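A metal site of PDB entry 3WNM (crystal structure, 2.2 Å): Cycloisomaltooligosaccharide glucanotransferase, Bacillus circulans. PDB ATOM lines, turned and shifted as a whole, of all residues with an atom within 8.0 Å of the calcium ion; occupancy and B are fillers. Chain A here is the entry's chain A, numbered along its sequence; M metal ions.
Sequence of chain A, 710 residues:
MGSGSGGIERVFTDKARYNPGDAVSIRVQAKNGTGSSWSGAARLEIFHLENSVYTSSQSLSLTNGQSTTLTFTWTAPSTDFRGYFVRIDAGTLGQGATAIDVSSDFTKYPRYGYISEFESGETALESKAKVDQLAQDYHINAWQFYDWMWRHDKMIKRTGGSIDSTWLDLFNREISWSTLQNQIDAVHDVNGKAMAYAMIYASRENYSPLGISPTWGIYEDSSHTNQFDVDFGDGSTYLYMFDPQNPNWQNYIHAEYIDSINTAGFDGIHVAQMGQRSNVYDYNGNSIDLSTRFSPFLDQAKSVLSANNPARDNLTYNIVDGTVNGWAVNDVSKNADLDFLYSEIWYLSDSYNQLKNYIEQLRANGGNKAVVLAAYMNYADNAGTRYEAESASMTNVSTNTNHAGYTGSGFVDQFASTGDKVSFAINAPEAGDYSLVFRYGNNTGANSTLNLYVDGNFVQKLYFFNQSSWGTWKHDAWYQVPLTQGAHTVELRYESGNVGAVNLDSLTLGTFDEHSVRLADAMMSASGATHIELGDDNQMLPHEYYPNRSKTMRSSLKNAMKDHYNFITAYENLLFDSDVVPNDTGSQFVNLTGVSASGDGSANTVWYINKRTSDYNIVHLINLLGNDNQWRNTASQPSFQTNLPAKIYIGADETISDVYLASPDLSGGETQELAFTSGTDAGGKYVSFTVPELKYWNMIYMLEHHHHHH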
ATOM      1  N   ARG A 386      18.173   0.746  14.612  1.00  0.00           N
ATOM      2  CA  ARG A 386      16.899   0.452  15.244  1.00  0.00           C
ATOM      3  C   ARG A 386      16.985   0.327  16.767  1.00  0.00           C
ATOM      4  O   ARG A 386      17.860  -0.361  17.279  1.00  0.00           O
ATOM      5  CB  ARG A 386      16.303  -0.820  14.669  1.00  0.00           C
ATOM      6  CG  ARG A 386      14.914  -1.117  15.222  1.00  0.00           C
ATOM      7  CD  ARG A 386      14.120  -1.988  14.279  1.00  0.00           C
ATOM      8  NE  ARG A 386      14.707  -3.317  14.246  1.00  0.00           N
ATOM      9  CZ  ARG A 386      14.758  -4.115  13.183  1.00  0.00           C
ATOM     10  NH1 ARG A 386      14.281  -3.745  12.007  1.00  0.00           N
ATOM     11  NH2 ARG A 386      15.317  -5.310  13.306  1.00  0.00           N
ATOM     12  N   TYR A 387      16.058   0.996  17.455  1.00  0.00           N
ATOM     13  CA  TYR A 387      15.850   0.877  18.891  1.00  0.00           C
ATOM     14  C   TYR A 387      14.465   0.298  19.124  1.00  0.00           C
ATOM     15  O   TYR A 387      13.445   0.947  18.840  1.00  0.00           O
ATOM     16  CB  TYR A 387      15.941   2.258  19.536  1.00  0.00           C
ATOM     17  CG  TYR A 387      17.298   2.907  19.408  1.00  0.00           C
ATOM     18  CD1 TYR A 387      17.619   3.711  18.322  1.00  0.00           C
ATOM     19  CD2 TYR A 387      18.273   2.709  20.385  1.00  0.00           C
ATOM     20  CE1 TYR A 387      18.884   4.312  18.210  1.00  0.00           C
ATOM     21  CE2 TYR A 387      19.526   3.296  20.284  1.00  0.00           C
ATOM     22  CZ  TYR A 387      19.831   4.093  19.198  1.00  0.00           C
ATOM     23  OH  TYR A 387      21.064   4.684  19.124  1.00  0.00           O
ATOM     24  N   GLU A 388      14.406  -0.937  19.620  1.00  0.00           N
ATOM     25  CA  GLU A 388      13.142  -1.620  19.862  1.00  0.00           C
ATOM     26  C   GLU A 388      12.377  -0.941  20.983  1.00  0.00           C
ATOM     27  O   GLU A 388      12.965  -0.577  22.021  1.00  0.00           O
ATOM     28  CB  GLU A 388      13.377  -3.097  20.182  1.00  0.00           C
ATOM     29  CG  GLU A 388      13.892  -3.915  18.997  1.00  0.00           C
ATOM     30  CD  GLU A 388      12.901  -3.999  17.830  1.00  0.00           C
ATOM     31  OE1 GLU A 388      11.773  -3.435  17.932  1.00  0.00           O
ATOM     32  OE2 GLU A 388      13.241  -4.631  16.810  1.00  0.00           O
ATOM     33  N   ALA A 389      11.075  -0.728  20.760  1.00  0.00           N
ATOM     34  CA  ALA A 389      10.218  -0.025  21.716  1.00  0.00           C
ATOM     35  C   ALA A 389      10.138  -0.798  23.060  1.00  0.00           C
ATOM     36  O   ALA A 389      10.141  -0.212  24.152  1.00  0.00           O
ATOM     37  CB  ALA A 389       8.836   0.198  21.133  1.00  0.00           C
ATOM     38  N   GLU A 390      10.092  -2.112  22.946  1.00  0.00           N
ATOM     39  CA  GLU A 390      10.069  -2.988  24.094  1.00  0.00           C
ATOM     40  C   GLU A 390      11.348  -2.941  24.932  1.00  0.00           C
ATOM     41  O   GLU A 390      11.343  -3.391  26.077  1.00  0.00           O
ATOM     42  CB  GLU A 390       9.726  -4.423  23.683  1.00  0.00           C
ATOM     43  CG  GLU A 390      10.714  -5.078  22.734  1.00  0.00           C
ATOM     44  CD  GLU A 390      10.392  -4.843  21.259  1.00  0.00           C
ATOM     45  OE1 GLU A 390       9.735  -3.816  20.929  1.00  0.00           O
ATOM     46  OE2 GLU A 390      10.788  -5.693  20.420  1.00  0.00           O
ATOM     47  N   SER A 391      12.424  -2.386  24.390  1.00  0.00           N
ATOM     48  CA  SER A 391      13.676  -2.240  25.127  1.00  0.00           C
ATOM     49  C   SER A 391      13.870  -0.827  25.665  1.00  0.00           C
ATOM     50  O   SER A 391      14.864  -0.547  26.272  1.00  0.00           O
ATOM     51  CB  SER A 391      14.868  -2.620  24.246  1.00  0.00           C
ATOM     52  OG  SER A 391      14.694  -3.939  23.788  1.00  0.00           O
ATOM     53  N   ASN A 400       3.840  -6.347  24.522  1.00  0.00           N
ATOM     54  CA  ASN A 400       3.029  -7.446  24.080  1.00  0.00           C
ATOM     55  C   ASN A 400       3.615  -8.096  22.834  1.00  0.00           C
ATOM     56  O   ASN A 400       4.623  -7.633  22.297  1.00  0.00           O
ATOM     57  CB  ASN A 400       1.587  -6.997  23.834  1.00  0.00           C
ATOM     58  CG  ASN A 400       0.593  -8.077  24.189  1.00  0.00           C
ATOM     59  OD1 ASN A 400       0.889  -9.280  24.041  1.00  0.00           O
ATOM     60  ND2 ASN A 400      -0.574  -7.684  24.672  1.00  0.00           N
ATOM     61  N   GLY A 405       4.150  -9.637  12.981  1.00  0.00           N
ATOM     62  CA  GLY A 405       4.807  -8.723  12.078  1.00  0.00           C
ATOM     63  C   GLY A 405       5.687  -7.680  12.757  1.00  0.00           C
ATOM     64  O   GLY A 405       6.247  -6.830  12.077  1.00  0.00           O
ATOM     65  N   TYR A 406       5.808  -7.739  14.078  1.00  0.00           N
ATOM     66  CA  TYR A 406       6.675  -6.848  14.837  1.00  0.00           C
ATOM     67  C   TYR A 406       8.107  -7.316  14.693  1.00  0.00           C
ATOM     68  O   TYR A 406       8.358  -8.498  14.459  1.00  0.00           O
ATOM     69  CB  TYR A 406       6.301  -6.827  16.327  1.00  0.00           C
ATOM     70  CG  TYR A 406       6.328  -8.204  16.992  1.00  0.00           C
ATOM     71  CD1 TYR A 406       7.518  -8.751  17.444  1.00  0.00           C
ATOM     72  CD2 TYR A 406       5.152  -8.950  17.158  1.00  0.00           C
ATOM     73  CE1 TYR A 406       7.548 -10.012  18.044  1.00  0.00           C
ATOM     74  CE2 TYR A 406       5.169 -10.208  17.754  1.00  0.00           C
ATOM     75  CZ  TYR A 406       6.373 -10.732  18.191  1.00  0.00           C
ATOM     76  OH  TYR A 406       6.411 -11.966  18.779  1.00  0.00           O
ATOM     77  N   THR A 407       9.042  -6.386  14.814  1.00  0.00           N
ATOM     78  CA  THR A 407      10.445  -6.712  14.900  1.00  0.00           C
ATOM     79  C   THR A 407      10.829  -6.874  16.377  1.00  0.00           C
ATOM     80  O   THR A 407      10.163  -6.325  17.289  1.00  0.00           O
ATOM     81  CB  THR A 407      11.318  -5.574  14.307  1.00  0.00           C
ATOM     82  OG1 THR A 407      11.097  -4.367  15.041  1.00  0.00           O
ATOM     83  CG2 THR A 407      10.955  -5.332  12.822  1.00  0.00           C
ATOM     84  N   GLY A 408      11.923  -7.595  16.609  1.00  0.00           N
ATOM     85  CA  GLY A 408      12.429  -7.816  17.959  1.00  0.00           C
ATOM     86  C   GLY A 408      11.548  -8.788  18.713  1.00  0.00           C
ATOM     87  O   GLY A 408      10.992  -9.718  18.135  1.00  0.00           O
ATOM     88  N   SER A 409      11.409  -8.569  20.013  1.00  0.00           N
ATOM     89  CA  SER A 409      10.743  -9.538  20.885  1.00  0.00           C
ATOM     90  C   SER A 409       9.286  -9.176  21.133  1.00  0.00           C
ATOM     91  O   SER A 409       8.576  -9.913  21.811  1.00  0.00           O
ATOM     92  CB  SER A 409      11.500  -9.641  22.214  1.00  0.00           C
ATOM     93  OG  SER A 409      11.366  -8.444  22.950  1.00  0.00           O
ATOM     94  N   GLY A 410       8.847  -8.043  20.597  1.00  0.00           N
ATOM     95  CA  GLY A 410       7.442  -7.656  20.663  1.00  0.00           C
ATOM     96  C   GLY A 410       7.262  -6.173  20.365  1.00  0.00           C
ATOM     97  O   GLY A 410       7.994  -5.600  19.567  1.00  0.00           O
ATOM     98  N   PHE A 411       6.293  -5.553  21.044  1.00  0.00           N
ATOM     99  CA  PHE A 411       5.996  -4.154  20.849  1.00  0.00           C
ATOM    100  C   PHE A 411       5.306  -3.570  22.086  1.00  0.00           C
ATOM    101  O   PHE A 411       4.968  -4.302  23.006  1.00  0.00           O
ATOM    102  CB  PHE A 411       5.077  -3.971  19.647  1.00  0.00           C
ATOM    103  CG  PHE A 411       3.808  -4.771  19.729  1.00  0.00           C
ATOM    104  CD1 PHE A 411       3.765  -6.077  19.247  1.00  0.00           C
ATOM    105  CD2 PHE A 411       2.654  -4.215  20.267  1.00  0.00           C
ATOM    106  CE1 PHE A 411       2.583  -6.816  19.315  1.00  0.00           C
ATOM    107  CE2 PHE A 411       1.474  -4.945  20.332  1.00  0.00           C
ATOM    108  CZ  PHE A 411       1.437  -6.250  19.858  1.00  0.00           C
ATOM    109  N   VAL A 412       5.079  -2.260  22.073  1.00  0.00           N
ATOM    110  CA  VAL A 412       4.372  -1.605  23.143  1.00  0.00           C
ATOM    111  C   VAL A 412       2.931  -1.361  22.714  1.00  0.00           C
ATOM    112  O   VAL A 412       2.695  -0.783  21.656  1.00  0.00           O
ATOM    113  CB  VAL A 412       5.076  -0.276  23.539  1.00  0.00           C
ATOM    114  CG1 VAL A 412       4.233   0.539  24.511  1.00  0.00           C
ATOM    115  CG2 VAL A 412       6.452  -0.589  24.144  1.00  0.00           C
ATOM    116  N   ARG A 439       7.921   2.886  13.743  1.00  0.00           N
ATOM    117  CA  ARG A 439       7.122   1.841  13.194  1.00  0.00           C
ATOM    118  C   ARG A 439       6.010   1.564  14.194  1.00  0.00           C
ATOM    119  O   ARG A 439       6.280   1.322  15.369  1.00  0.00           O
ATOM    120  CB  ARG A 439       7.956   0.592  12.962  1.00  0.00           C
ATOM    121  CG  ARG A 439       7.233  -0.447  12.142  1.00  0.00           C
ATOM    122  CD  ARG A 439       8.151  -1.582  11.749  1.00  0.00           C
ATOM    123  NE  ARG A 439       7.555  -2.423  10.730  1.00  0.00           N
ATOM    124  CZ  ARG A 439       7.111  -3.667  10.906  1.00  0.00           C
ATOM    125  NH1 ARG A 439       7.159  -4.283  12.084  1.00  0.00           N
ATOM    126  NH2 ARG A 439       6.605  -4.322   9.882  1.00  0.00           N
ATOM    127  N   TRP A 473       1.641  -3.096  10.164  1.00  0.00           N
ATOM    128  CA  TRP A 473       2.649  -2.146  10.631  1.00  0.00           C
ATOM    129  C   TRP A 473       3.073  -1.159   9.544  1.00  0.00           C
ATOM    130  O   TRP A 473       3.238  -1.544   8.397  1.00  0.00           O
ATOM    131  CB  TRP A 473       3.864  -2.906  11.149  1.00  0.00           C
ATOM    132  CG  TRP A 473       3.484  -3.851  12.233  1.00  0.00           C
ATOM    133  CD1 TRP A 473       3.186  -5.178  12.094  1.00  0.00           C
ATOM    134  CD2 TRP A 473       3.352  -3.553  13.625  1.00  0.00           C
ATOM    135  NE1 TRP A 473       2.882  -5.719  13.325  1.00  0.00           N
ATOM    136  CE2 TRP A 473       2.978  -4.746  14.280  1.00  0.00           C
ATOM    137  CE3 TRP A 473       3.531  -2.394  14.379  1.00  0.00           C
ATOM    138  CZ2 TRP A 473       2.783  -4.815  15.658  1.00  0.00           C
ATOM    139  CZ3 TRP A 473       3.327  -2.456  15.737  1.00  0.00           C
ATOM    140  CH2 TRP A 473       2.957  -3.646  16.376  1.00  0.00           C
ATOM    141  N   LEU A 504       3.413   0.548  19.335  1.00  0.00           N
ATOM    142  CA  LEU A 504       4.699   1.109  18.939  1.00  0.00           C
ATOM    143  C   LEU A 504       5.729   0.007  18.923  1.00  0.00           C
ATOM    144  O   LEU A 504       6.001  -0.628  19.942  1.00  0.00           O
ATOM    145  CB  LEU A 504       5.116   2.197  19.886  1.00  0.00           C
ATOM    146  CG  LEU A 504       6.323   3.045  19.524  1.00  0.00           C
ATOM    147  CD1 LEU A 504       6.169   3.808  18.204  1.00  0.00           C
ATOM    148  CD2 LEU A 504       6.536   4.010  20.672  1.00  0.00           C
ATOM    149  N   ASP A 505       6.292  -0.221  17.754  1.00  0.00           N
ATOM    150  CA  ASP A 505       7.214  -1.320  17.564  1.00  0.00           C
ATOM    151  C   ASP A 505       8.650  -0.894  17.842  1.00  0.00           C
ATOM    152  O   ASP A 505       9.421  -1.623  18.464  1.00  0.00           O
ATOM    153  CB  ASP A 505       7.078  -1.829  16.137  1.00  0.00           C
ATOM    154  CG  ASP A 505       7.755  -3.163  15.925  1.00  0.00           C
ATOM    155  OD1 ASP A 505       8.069  -3.855  16.913  1.00  0.00           O
ATOM    156  OD2 ASP A 505       7.925  -3.545  14.763  1.00  0.00           O
ATOM    157  N   SER A 506       9.012   0.298  17.372  1.00  0.00           N
ATOM    158  CA  SER A 506      10.387   0.701  17.385  1.00  0.00           C
ATOM    159  C   SER A 506      10.561   2.138  16.913  1.00  0.00           C
ATOM    160  O   SER A 506       9.661   2.731  16.313  1.00  0.00           O
ATOM    161  CB  SER A 506      11.189  -0.195  16.435  1.00  0.00           C
ATOM    162  OG  SER A 506      10.794   0.002  15.097  1.00  0.00           O
ATOM    163  N   LEU A 507      11.733   2.681  17.208  1.00  0.00           N
ATOM    164  CA  LEU A 507      12.227   3.913  16.671  1.00  0.00           C
ATOM    165  C   LEU A 507      13.439   3.561  15.820  1.00  0.00           C
ATOM    166  O   LEU A 507      14.237   2.691  16.188  1.00  0.00           O
ATOM    167  CB  LEU A 507      12.665   4.836  17.801  1.00  0.00           C
ATOM    168  CG  LEU A 507      13.663   5.950  17.448  1.00  0.00           C
ATOM    169  CD1 LEU A 507      13.030   7.006  16.541  1.00  0.00           C
ATOM    170  CD2 LEU A 507      14.169   6.580  18.716  1.00  0.00           C
HETATM  171 CA    CA M   1       9.638  -4.294  18.435  1.00  0.00          CA
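Of the 21 residues printed, 5 come within 4 Å of the calcium ion.
The nearest printed residue that does not touch the calcium ion is Phe 411 (4.4 Å).
The calcium ion is bound by OD1 of Asp 505.
The calcium ion is bound by the side-chain carboxylate (OE1) of Glu 388.
O of Gly 410 is bound to the calcium ion (2.4 Å).
The calcium ion is bound by O of Thr 407 (2.4 Å).
The calcium ion is bound by the side-chain carboxylate (OE1) of Glu 390 (2.5 Å).
The backbone carbonyl oxygen (O) of Asp 505 is bound to the calcium ion, 2.7 Å away.
OE2 of Glu 390 is bound to the calcium ion (2.7 Å).
The backbone NH (N) of Gly 408 lies within hydrogen-bond range of the side-chain carboxylate (OE2) of Glu 388.
O of Asp 505 lies close to N of Ala 389, 3.0 Å away.
The side-chain carboxylate (OD2) of Asp 505 lies within salt-bridge range of the guanidinium group (NH1) of Arg 439.
The guanidinium group of Arg 386 is in salt-bridge range of the side-chain carboxylate of Glu 388, 3.2 Å away.
N of Ser 409 lies close to OE2 of Glu 390 (3.0 Å).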
